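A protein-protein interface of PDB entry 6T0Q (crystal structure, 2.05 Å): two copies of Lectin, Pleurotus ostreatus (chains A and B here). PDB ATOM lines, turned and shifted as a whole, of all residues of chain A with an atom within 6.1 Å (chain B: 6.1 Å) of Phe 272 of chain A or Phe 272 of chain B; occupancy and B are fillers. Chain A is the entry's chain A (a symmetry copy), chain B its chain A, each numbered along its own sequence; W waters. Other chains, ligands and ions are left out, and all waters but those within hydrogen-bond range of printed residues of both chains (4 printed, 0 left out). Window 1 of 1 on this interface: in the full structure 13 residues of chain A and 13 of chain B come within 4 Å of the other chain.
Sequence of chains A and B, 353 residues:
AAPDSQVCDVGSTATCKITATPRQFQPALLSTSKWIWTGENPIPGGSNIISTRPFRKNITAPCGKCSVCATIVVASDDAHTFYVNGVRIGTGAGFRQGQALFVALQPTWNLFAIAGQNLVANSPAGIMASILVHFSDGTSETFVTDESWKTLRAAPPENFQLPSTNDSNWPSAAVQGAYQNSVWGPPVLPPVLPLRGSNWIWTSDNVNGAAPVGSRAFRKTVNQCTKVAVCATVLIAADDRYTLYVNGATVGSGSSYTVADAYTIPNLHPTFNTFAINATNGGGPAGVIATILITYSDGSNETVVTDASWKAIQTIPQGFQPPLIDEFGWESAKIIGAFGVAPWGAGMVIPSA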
ATOM      1  N   THR A 221      10.805  -9.842 -14.875  1.00  0.00           N
ATOM      2  CA  THR A 221      10.339  -9.610 -16.234  1.00  0.00           C
ATOM      3  C   THR A 221      10.156 -10.935 -16.959  1.00  0.00           C
ATOM      4  O   THR A 221      10.995 -11.831 -16.852  1.00  0.00           O
ATOM      5  CB  THR A 221      11.333  -8.736 -17.005  1.00  0.00           C
ATOM      6  OG1 THR A 221      11.407  -7.458 -16.373  1.00  0.00           O
ATOM      7  CG2 THR A 221      10.895  -8.554 -18.465  1.00  0.00           C
ATOM      8  N   VAL A 222       9.060 -11.063 -17.695  1.00  0.00           N
ATOM      9  CA  VAL A 222       8.861 -12.184 -18.606  1.00  0.00           C
ATOM     10  C   VAL A 222       8.813 -11.614 -20.018  1.00  0.00           C
ATOM     11  O   VAL A 222       8.046 -10.684 -20.290  1.00  0.00           O
ATOM     12  CB  VAL A 222       7.583 -12.980 -18.271  1.00  0.00           C
ATOM     13  CG1 VAL A 222       7.416 -14.153 -19.238  1.00  0.00           C
ATOM     14  CG2 VAL A 222       7.651 -13.491 -16.817  1.00  0.00           C
ATOM     15  N   ASN A 223       9.640 -12.160 -20.910  1.00  0.00           N
ATOM     16  CA  ASN A 223       9.733 -11.590 -22.259  1.00  0.00           C
ATOM     17  C   ASN A 223      10.007 -12.745 -23.225  1.00  0.00           C
ATOM     18  O   ASN A 223      11.145 -13.031 -23.592  1.00  0.00           O
ATOM     19  CB  ASN A 223      10.812 -10.504 -22.324  1.00  0.00           C
ATOM     20  CG  ASN A 223      11.078  -9.993 -23.736  1.00  0.00           C
ATOM     21  OD1 ASN A 223      12.223  -9.681 -24.075  1.00  0.00           O
ATOM     22  ND2 ASN A 223      10.034  -9.890 -24.557  1.00  0.00           N
ATOM     23  N   GLN A 224       8.934 -13.434 -23.626  1.00  0.00           N
ATOM     24  CA  GLN A 224       9.022 -14.463 -24.667  1.00  0.00           C
ATOM     25  C   GLN A 224       8.706 -13.783 -25.996  1.00  0.00           C
ATOM     26  O   GLN A 224       7.556 -13.722 -26.427  1.00  0.00           O
ATOM     27  CB  GLN A 224       8.062 -15.617 -24.381  1.00  0.00           C
ATOM     28  CG  GLN A 224       8.207 -16.246 -22.996  1.00  0.00           C
ATOM     29  CD  GLN A 224       9.462 -17.094 -22.845  1.00  0.00           C
ATOM     30  OE1 GLN A 224      10.116 -17.436 -23.827  1.00  0.00           O
ATOM     31  NE2 GLN A 224       9.794 -17.445 -21.603  1.00  0.00           N
ATOM     32  N   ASN A 247       3.819  -3.719 -15.382  1.00  0.00           N
ATOM     33  CA  ASN A 247       4.162  -2.704 -16.384  1.00  0.00           C
ATOM     34  C   ASN A 247       3.927  -1.289 -15.858  1.00  0.00           C
ATOM     35  O   ASN A 247       3.450  -0.406 -16.573  1.00  0.00           O
ATOM     36  CB  ASN A 247       3.393  -2.951 -17.678  1.00  0.00           C
ATOM     37  CG  ASN A 247       3.703  -4.305 -18.260  1.00  0.00           C
ATOM     38  OD1 ASN A 247       4.849  -4.758 -18.196  1.00  0.00           O
ATOM     39  ND2 ASN A 247       2.684  -4.982 -18.797  1.00  0.00           N
ATOM     40  N   LEU A 268      -2.317  -8.006 -20.528  1.00  0.00           N
ATOM     41  CA  LEU A 268      -0.864  -8.073 -20.651  1.00  0.00           C
ATOM     42  C   LEU A 268      -0.396  -7.477 -21.976  1.00  0.00           C
ATOM     43  O   LEU A 268      -1.116  -7.483 -22.977  1.00  0.00           O
ATOM     44  CB  LEU A 268      -0.387  -9.520 -20.566  1.00  0.00           C
ATOM     45  CG  LEU A 268      -0.534 -10.271 -19.248  1.00  0.00           C
ATOM     46  CD1 LEU A 268      -0.021 -11.690 -19.435  1.00  0.00           C
ATOM     47  CD2 LEU A 268       0.260  -9.543 -18.174  1.00  0.00           C
ATOM     48  N   HIS A 269       0.823  -6.942 -21.972  1.00  0.00           N
ATOM     49  CA  HIS A 269       1.512  -6.679 -23.223  1.00  0.00           C
ATOM     50  C   HIS A 269       1.796  -8.016 -23.906  1.00  0.00           C
ATOM     51  O   HIS A 269       2.035  -9.019 -23.231  1.00  0.00           O
ATOM     52  CB  HIS A 269       2.820  -5.924 -22.967  1.00  0.00           C
ATOM     53  CG  HIS A 269       3.529  -5.490 -24.212  1.00  0.00           C
ATOM     54  ND1 HIS A 269       4.461  -6.280 -24.853  1.00  0.00           N
ATOM     55  CD2 HIS A 269       3.442  -4.346 -24.936  1.00  0.00           C
ATOM     56  CE1 HIS A 269       4.920  -5.640 -25.918  1.00  0.00           C
ATOM     57  NE2 HIS A 269       4.316  -4.466 -25.993  1.00  0.00           N
ATOM     58  N   PRO A 270       1.746  -8.069 -25.241  1.00  0.00           N
ATOM     59  CA  PRO A 270       1.878  -9.371 -25.915  1.00  0.00           C
ATOM     60  C   PRO A 270       3.241 -10.031 -25.762  1.00  0.00           C
ATOM     61  O   PRO A 270       3.318 -11.262 -25.879  1.00  0.00           O
ATOM     62  CB  PRO A 270       1.573  -9.043 -27.389  1.00  0.00           C
ATOM     63  CG  PRO A 270       1.694  -7.571 -27.499  1.00  0.00           C
ATOM     64  CD  PRO A 270       1.316  -7.011 -26.170  1.00  0.00           C
ATOM     65  N   THR A 271       4.324  -9.280 -25.523  1.00  0.00           N
ATOM     66  CA  THR A 271       5.649  -9.896 -25.488  1.00  0.00           C
ATOM     67  C   THR A 271       6.507  -9.557 -24.272  1.00  0.00           C
ATOM     68  O   THR A 271       7.441 -10.314 -23.988  1.00  0.00           O
ATOM     69  CB  THR A 271       6.448  -9.539 -26.752  1.00  0.00           C
ATOM     70  OG1 THR A 271       6.568  -8.113 -26.868  1.00  0.00           O
ATOM     71  CG2 THR A 271       5.771 -10.110 -27.994  1.00  0.00           C
ATOM     72  N   PHE A 272       6.234  -8.477 -23.541  1.00  0.00           N
ATOM     73  CA  PHE A 272       7.148  -8.022 -22.496  1.00  0.00           C
ATOM     74  C   PHE A 272       6.327  -7.526 -21.315  1.00  0.00           C
ATOM     75  O   PHE A 272       5.585  -6.550 -21.450  1.00  0.00           O
ATOM     76  CB  PHE A 272       8.069  -6.909 -23.042  1.00  0.00           C
ATOM     77  CG  PHE A 272       9.193  -6.493 -22.110  1.00  0.00           C
ATOM     78  CD1 PHE A 272       8.950  -5.695 -21.000  1.00  0.00           C
ATOM     79  CD2 PHE A 272      10.509  -6.856 -22.389  1.00  0.00           C
ATOM     80  CE1 PHE A 272       9.997  -5.296 -20.157  1.00  0.00           C
ATOM     81  CE2 PHE A 272      11.555  -6.458 -21.564  1.00  0.00           C
ATOM     82  CZ  PHE A 272      11.300  -5.677 -20.444  1.00  0.00           C
ATOM     83  N   ASN A 273       6.476  -8.174 -20.154  1.00  0.00           N
ATOM     84  CA  ASN A 273       5.732  -7.793 -18.957  1.00  0.00           C
ATOM     85  C   ASN A 273       6.628  -7.839 -17.733  1.00  0.00           C
ATOM     86  O   ASN A 273       7.320  -8.836 -17.507  1.00  0.00           O
ATOM     87  CB  ASN A 273       4.519  -8.711 -18.753  1.00  0.00           C
ATOM     88  CG  ASN A 273       3.494  -8.539 -19.845  1.00  0.00           C
ATOM     89  OD1 ASN A 273       2.703  -7.598 -19.817  1.00  0.00           O
ATOM     90  ND2 ASN A 273       3.521  -9.424 -20.831  1.00  0.00           N
ATOM     91  N   THR A 274       6.581  -6.774 -16.931  1.00  0.00           N
ATOM     92  CA  THR A 274       7.412  -6.632 -15.740  1.00  0.00           C
ATOM     93  C   THR A 274       6.529  -6.565 -14.501  1.00  0.00           C
ATOM     94  O   THR A 274       5.670  -5.682 -14.391  1.00  0.00           O
ATOM     95  CB  THR A 274       8.288  -5.378 -15.816  1.00  0.00           C
ATOM     96  OG1 THR A 274       9.294  -5.551 -16.821  1.00  0.00           O
ATOM     97  CG2 THR A 274       8.971  -5.138 -14.463  1.00  0.00           C
ATOM     98  N   PRO A 323       8.694  -0.617 -16.546  1.00  0.00           N
ATOM     99  CA  PRO A 323       9.210  -1.873 -17.116  1.00  0.00           C
ATOM    100  C   PRO A 323      10.653  -1.821 -17.592  1.00  0.00           C
ATOM    101  O   PRO A 323      11.359  -2.831 -17.455  1.00  0.00           O
ATOM    102  CB  PRO A 323       8.251  -2.144 -18.286  1.00  0.00           C
ATOM    103  CG  PRO A 323       7.607  -0.814 -18.583  1.00  0.00           C
ATOM    104  CD  PRO A 323       7.501  -0.128 -17.259  1.00  0.00           C
ATOM    105  N   LEU A 324      11.120  -0.702 -18.156  1.00  0.00           N
ATOM    106  CA  LEU A 324      12.417  -0.682 -18.829  1.00  0.00           C
ATOM    107  C   LEU A 324      13.507   0.046 -18.045  1.00  0.00           C
ATOM    108  O   LEU A 324      14.414   0.635 -18.643  1.00  0.00           O
ATOM    109  CB  LEU A 324      12.296  -0.060 -20.218  1.00  0.00           C
ATOM    110  CG  LEU A 324      11.487  -0.809 -21.271  1.00  0.00           C
ATOM    111  CD1 LEU A 324      11.730  -0.175 -22.639  1.00  0.00           C
ATOM    112  CD2 LEU A 324      11.842  -2.280 -21.301  1.00  0.00           C
ATOM    113  N   THR B 221       9.470  -1.143 -32.529  1.00  0.00           N
ATOM    114  CA  THR B 221      10.091  -1.824 -31.402  1.00  0.00           C
ATOM    115  C   THR B 221      11.093  -2.855 -31.900  1.00  0.00           C
ATOM    116  O   THR B 221      10.821  -3.587 -32.852  1.00  0.00           O
ATOM    117  CB  THR B 221       9.032  -2.513 -30.535  1.00  0.00           C
ATOM    118  OG1 THR B 221       8.168  -1.519 -29.987  1.00  0.00           O
ATOM    119  CG2 THR B 221       9.683  -3.305 -29.391  1.00  0.00           C
ATOM    120  N   VAL B 222      12.254  -2.912 -31.259  1.00  0.00           N
ATOM    121  CA  VAL B 222      13.216  -3.984 -31.486  1.00  0.00           C
ATOM    122  C   VAL B 222      13.337  -4.763 -30.184  1.00  0.00           C
ATOM    123  O   VAL B 222      13.575  -4.175 -29.123  1.00  0.00           O
ATOM    124  CB  VAL B 222      14.583  -3.443 -31.954  1.00  0.00           C
ATOM    125  CG1 VAL B 222      15.559  -4.595 -32.195  1.00  0.00           C
ATOM    126  CG2 VAL B 222      14.404  -2.615 -33.243  1.00  0.00           C
ATOM    127  N   ASN B 223      13.159  -6.083 -30.260  1.00  0.00           N
ATOM    128  CA  ASN B 223      13.147  -6.887 -29.032  1.00  0.00           C
ATOM    129  C   ASN B 223      13.750  -8.251 -29.374  1.00  0.00           C
ATOM    130  O   ASN B 223      13.048  -9.220 -29.659  1.00  0.00           O
ATOM    131  CB  ASN B 223      11.729  -6.999 -28.462  1.00  0.00           C
ATOM    132  CG  ASN B 223      11.621  -7.963 -27.285  1.00  0.00           C
ATOM    133  OD1 ASN B 223      10.608  -8.651 -27.142  1.00  0.00           O
ATOM    134  ND2 ASN B 223      12.645  -8.007 -26.434  1.00  0.00           N
ATOM    135  N   GLN B 224      15.085  -8.316 -29.364  1.00  0.00           N
ATOM    136  CA  GLN B 224      15.798  -9.588 -29.517  1.00  0.00           C
ATOM    137  C   GLN B 224      16.063 -10.125 -28.114  1.00  0.00           C
ATOM    138  O   GLN B 224      17.095  -9.843 -27.506  1.00  0.00           O
ATOM    139  CB  GLN B 224      17.093  -9.400 -30.305  1.00  0.00           C
ATOM    140  CG  GLN B 224      16.929  -8.714 -31.660  1.00  0.00           C
ATOM    141  CD  GLN B 224      16.278  -9.601 -32.712  1.00  0.00           C
ATOM    142  OE1 GLN B 224      16.164 -10.812 -32.536  1.00  0.00           O
ATOM    143  NE2 GLN B 224      15.856  -8.995 -33.821  1.00  0.00           N
ATOM    144  N   ASN B 247      12.306   4.658 -25.831  1.00  0.00           N
ATOM    145  CA  ASN B 247      11.776   4.183 -24.550  1.00  0.00           C
ATOM    146  C   ASN B 247      11.125   5.314 -23.754  1.00  0.00           C
ATOM    147  O   ASN B 247      11.262   5.406 -22.533  1.00  0.00           O
ATOM    148  CB  ASN B 247      12.870   3.494 -23.742  1.00  0.00           C
ATOM    149  CG  ASN B 247      13.443   2.310 -24.477  1.00  0.00           C
ATOM    150  OD1 ASN B 247      12.707   1.586 -25.152  1.00  0.00           O
ATOM    151  ND2 ASN B 247      14.762   2.123 -24.388  1.00  0.00           N
ATOM    152  N   LEU B 268      20.856   2.007 -24.286  1.00  0.00           N
ATOM    153  CA  LEU B 268      19.722   1.159 -24.639  1.00  0.00           C
ATOM    154  C   LEU B 268      19.380   0.196 -23.503  1.00  0.00           C
ATOM    155  O   LEU B 268      20.239  -0.193 -22.709  1.00  0.00           O
ATOM    156  CB  LEU B 268      20.030   0.349 -25.895  1.00  0.00           C
ATOM    157  CG  LEU B 268      20.185   1.077 -27.225  1.00  0.00           C
ATOM    158  CD1 LEU B 268      20.519   0.059 -28.304  1.00  0.00           C
ATOM    159  CD2 LEU B 268      18.885   1.801 -27.546  1.00  0.00           C
ATOM    160  N   HIS B 269      18.106  -0.176 -23.423  1.00  0.00           N
ATOM    161  CA  HIS B 269      17.729  -1.339 -22.640  1.00  0.00           C
ATOM    162  C   HIS B 269      18.341  -2.578 -23.294  1.00  0.00           C
ATOM    163  O   HIS B 269      18.472  -2.633 -24.518  1.00  0.00           O
ATOM    164  CB  HIS B 269      16.206  -1.472 -22.573  1.00  0.00           C
ATOM    165  CG  HIS B 269      15.726  -2.566 -21.670  1.00  0.00           C
ATOM    166  ND1 HIS B 269      15.518  -3.857 -22.109  1.00  0.00           N
ATOM    167  CD2 HIS B 269      15.413  -2.562 -20.350  1.00  0.00           C
ATOM    168  CE1 HIS B 269      15.095  -4.602 -21.099  1.00  0.00           C
ATOM    169  NE2 HIS B 269      15.027  -3.841 -20.020  1.00  0.00           N
ATOM    170  N   PRO B 270      18.756  -3.573 -22.502  1.00  0.00           N
ATOM    171  CA  PRO B 270      19.474  -4.712 -23.096  1.00  0.00           C
ATOM    172  C   PRO B 270      18.639  -5.570 -24.037  1.00  0.00           C
ATOM    173  O   PRO B 270      19.222  -6.235 -24.904  1.00  0.00           O
ATOM    174  CB  PRO B 270      19.944  -5.516 -21.869  1.00  0.00           C
ATOM    175  CG  PRO B 270      19.137  -5.014 -20.734  1.00  0.00           C
ATOM    176  CD  PRO B 270      18.823  -3.587 -21.031  1.00  0.00           C
ATOM    177  N   THR B 271      17.307  -5.604 -23.904  1.00  0.00           N
ATOM    178  CA  THR B 271      16.511  -6.511 -24.730  1.00  0.00           C
ATOM    179  C   THR B 271      15.317  -5.884 -25.443  1.00  0.00           C
ATOM    180  O   THR B 271      14.851  -6.471 -26.425  1.00  0.00           O
ATOM    181  CB  THR B 271      16.001  -7.698 -23.896  1.00  0.00           C
ATOM    182  OG1 THR B 271      15.219  -7.220 -22.791  1.00  0.00           O
ATOM    183  CG2 THR B 271      17.168  -8.537 -23.386  1.00  0.00           C
ATOM    184  N   PHE B 272      14.812  -4.728 -25.013  1.00  0.00           N
ATOM    185  CA  PHE B 272      13.559  -4.205 -25.552  1.00  0.00           C
ATOM    186  C   PHE B 272      13.681  -2.696 -25.692  1.00  0.00           C
ATOM    187  O   PHE B 272      13.841  -1.998 -24.687  1.00  0.00           O
ATOM    188  CB  PHE B 272      12.382  -4.586 -24.626  1.00  0.00           C
ATOM    189  CG  PHE B 272      11.004  -4.271 -25.178  1.00  0.00           C
ATOM    190  CD1 PHE B 272      10.517  -2.970 -25.198  1.00  0.00           C
ATOM    191  CD2 PHE B 272      10.172  -5.296 -25.620  1.00  0.00           C
ATOM    192  CE1 PHE B 272       9.233  -2.691 -25.689  1.00  0.00           C
ATOM    193  CE2 PHE B 272       8.894  -5.030 -26.100  1.00  0.00           C
ATOM    194  CZ  PHE B 272       8.423  -3.724 -26.136  1.00  0.00           C
ATOM    195  N   ASN B 273      13.581  -2.188 -26.925  1.00  0.00           N
ATOM    196  CA  ASN B 273      13.695  -0.755 -27.181  1.00  0.00           C
ATOM    197  C   ASN B 273      12.659  -0.310 -28.197  1.00  0.00           C
ATOM    198  O   ASN B 273      12.528  -0.924 -29.261  1.00  0.00           O
ATOM    199  CB  ASN B 273      15.103  -0.398 -27.676  1.00  0.00           C
ATOM    200  CG  ASN B 273      16.146  -0.625 -26.613  1.00  0.00           C
ATOM    201  OD1 ASN B 273      16.322   0.204 -25.722  1.00  0.00           O
ATOM    202  ND2 ASN B 273      16.823  -1.762 -26.676  1.00  0.00           N
ATOM    203  N   THR B 274      11.957   0.779 -27.882  1.00  0.00           N
ATOM    204  CA  THR B 274      10.890   1.315 -28.721  1.00  0.00           C
ATOM    205  C   THR B 274      11.264   2.712 -29.201  1.00  0.00           C
ATOM    206  O   THR B 274      11.503   3.610 -28.385  1.00  0.00           O
ATOM    207  CB  THR B 274       9.559   1.370 -27.965  1.00  0.00           C
ATOM    208  OG1 THR B 274       9.075   0.040 -27.741  1.00  0.00           O
ATOM    209  CG2 THR B 274       8.523   2.144 -28.792  1.00  0.00           C
ATOM    210  N   PRO B 323       7.031   2.709 -24.070  1.00  0.00           N
ATOM    211  CA  PRO B 323       7.381   1.474 -24.792  1.00  0.00           C
ATOM    212  C   PRO B 323       6.287   0.420 -24.836  1.00  0.00           C
ATOM    213  O   PRO B 323       6.173  -0.274 -25.858  1.00  0.00           O
ATOM    214  CB  PRO B 323       8.612   0.962 -24.029  1.00  0.00           C
ATOM    215  CG  PRO B 323       8.556   1.646 -22.686  1.00  0.00           C
ATOM    216  CD  PRO B 323       7.957   2.988 -22.958  1.00  0.00           C
ATOM    217  N   LEU B 324       5.488   0.255 -23.777  1.00  0.00           N
ATOM    218  CA  LEU B 324       4.581  -0.887 -23.686  1.00  0.00           C
ATOM    219  C   LEU B 324       3.113  -0.527 -23.906  1.00  0.00           C
ATOM    220  O   LEU B 324       2.224  -1.170 -23.336  1.00  0.00           O
ATOM    221  CB  LEU B 324       4.731  -1.591 -22.339  1.00  0.00           C
ATOM    222  CG  LEU B 324       6.047  -2.301 -22.044  1.00  0.00           C
ATOM    223  CD1 LEU B 324       5.884  -3.165 -20.795  1.00  0.00           C
ATOM    224  CD2 LEU B 324       6.497  -3.145 -23.216  1.00  0.00           C
HETATM  225  O   HOH W   1       8.535  -8.109 -28.741  1.00  0.00           O
HETATM  226  O   HOH W   2       3.842  -1.738 -27.141  1.00  0.00           O
HETATM  227  O   HOH W   3      14.079  -9.600 -22.152  1.00  0.00           O
HETATM  228  O   HOH W   4      14.351  -3.265 -17.157  1.00  0.00           O
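The side-chain amide oxygen (OD1) of Asn 223 of chain B sits at hydrogen-bond distance from the side-chain amide nitrogen (ND2) of Asn 223 of chain A (2.9 Å).
O of Thr 274 of chain B sits at hydrogen-bond distance from N of Asn 247 of chain B (2.9 Å).
The side-chain amide nitrogen (ND2) of Asn 223 of chain B lies within hydrogen-bond range of the backbone carbonyl oxygen (O) of Thr 271 of chain B (2.7 Å).
The backbone carbonyl oxygen of Pro 323 of chain A sits at hydrogen-bond distance from the side-chain hydroxyl of Thr 274 of chain A, at 3.5 Å.
N of Gln 224 of chain B is in hydrogen-bond range of O of Thr 271 of chain B.
The side-chain amide nitrogen of Asn 247 of chain A sits at hydrogen-bond distance from the side-chain amide oxygen of Asn 273 of chain A.
O of His 269 of chain A lies within hydrogen-bond range of ND2 of Asn 273 of chain A (2.9 Å).
Water W1 bridges the side-chain amide oxygen (OD1) of Asn 223 of chain B and the side-chain hydroxyl (OG1) of Thr 271 of chain A.
Water W3 lies within hydrogen-bond range of the side-chain amide oxygen of Asn 223 of chain A and the side-chain hydroxyl of Thr 271 of chain B.
Water W4 lies within hydrogen-bond range of NE2 of His 269 of chain B (3.0 Å) and O of Pro 323 of chain A (3.0 Å).
Water W2 bridges a ring nitrogen (NE2) of His 269 of chain A (3.0 Å) and the backbone carbonyl oxygen of Pro 323 of chain B (3.0 Å).
Asn 223 of chain B touches its own counterpart, Asn 223 of chain A.
Asn 247 of chain A touches Leu 324 of chain B, and with the chains exchanged Leu 324 of chain A touches Asn 247 of chain B.
His 269 of chain A touches Leu 324 of chain B, and with the chains exchanged Leu 324 of chain A touches His 269 of chain B.
Phe 272 of chain A touches Leu 324 of chain B, and with the chains exchanged Leu 324 of chain A touches Phe 272 of chain B.
14 positions are printed for both chains.
Asn 247 of chain A touches Leu 324 of chain B.
His 269 of chain A touches Phe 272 of chain B (CE1 to CZ, 3.999 Å).
His 269 of chain A touches Leu 324 of chain B (CD2 to CD2, 3.7 Å).
His 269 of chain B touches Phe 272 of chain A (CE1 to CZ, 3.998 Å).
Phe 272 of chain A touches Phe 272 of chain B (CD2 to CD2, 3.6 Å).
Phe 272 of chain A touches Leu 324 of chain B (O to CD1, 3.5 Å).
Pro 323 of chain A touches Leu 324 of chain B.
Leu 324 of chain A touches Asn 247 of chain B.
Leu 324 of chain A touches His 269 of chain B.
Pro 323 of chain B touches Leu 324 of chain A.
Hydrophobic or aromatic side chains of chain B that line the printed part of chain A: His 269, Phe 272, Pro 323 and Leu 324.
Of the 14 printed residues of chain A, 7 touch a printed residue of chain B.
Along chain A the printed residues that touch a printed residue of chain B span positions 223 to 324.
Among the printed residues, 14 pairs touch across the chains.
Printed residues of chain B within 4 Å of Asn 247 of chain A: Leu 324 (3.2 Å).
Of the printed residues of chain B, Phe 272 of chain A touches His 269 (3.998 Å), Thr 271 (3.9 Å), Phe 272 (3.6 Å) and Leu 324 (3.5 Å).
Printed residues of chain B within 4 Å of Leu 324 of chain A: Asn 247 (3.2 Å), His 269 (3.7 Å), Phe 272 (3.5 Å) and Pro 323 (3.6 Å).
Printed residues of chain A within 4 Å of Phe 272 of chain B: His 269, Thr 271, Phe 272 and Leu 324.
The nearest printed residue of chain B that does not touch Phe 272 of chain A is Asn 223 of chain B (4.7 Å).
The nearest printed residue of chain A that does not touch Pro 323 of chain B is His 269 of chain A (4.6 Å).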
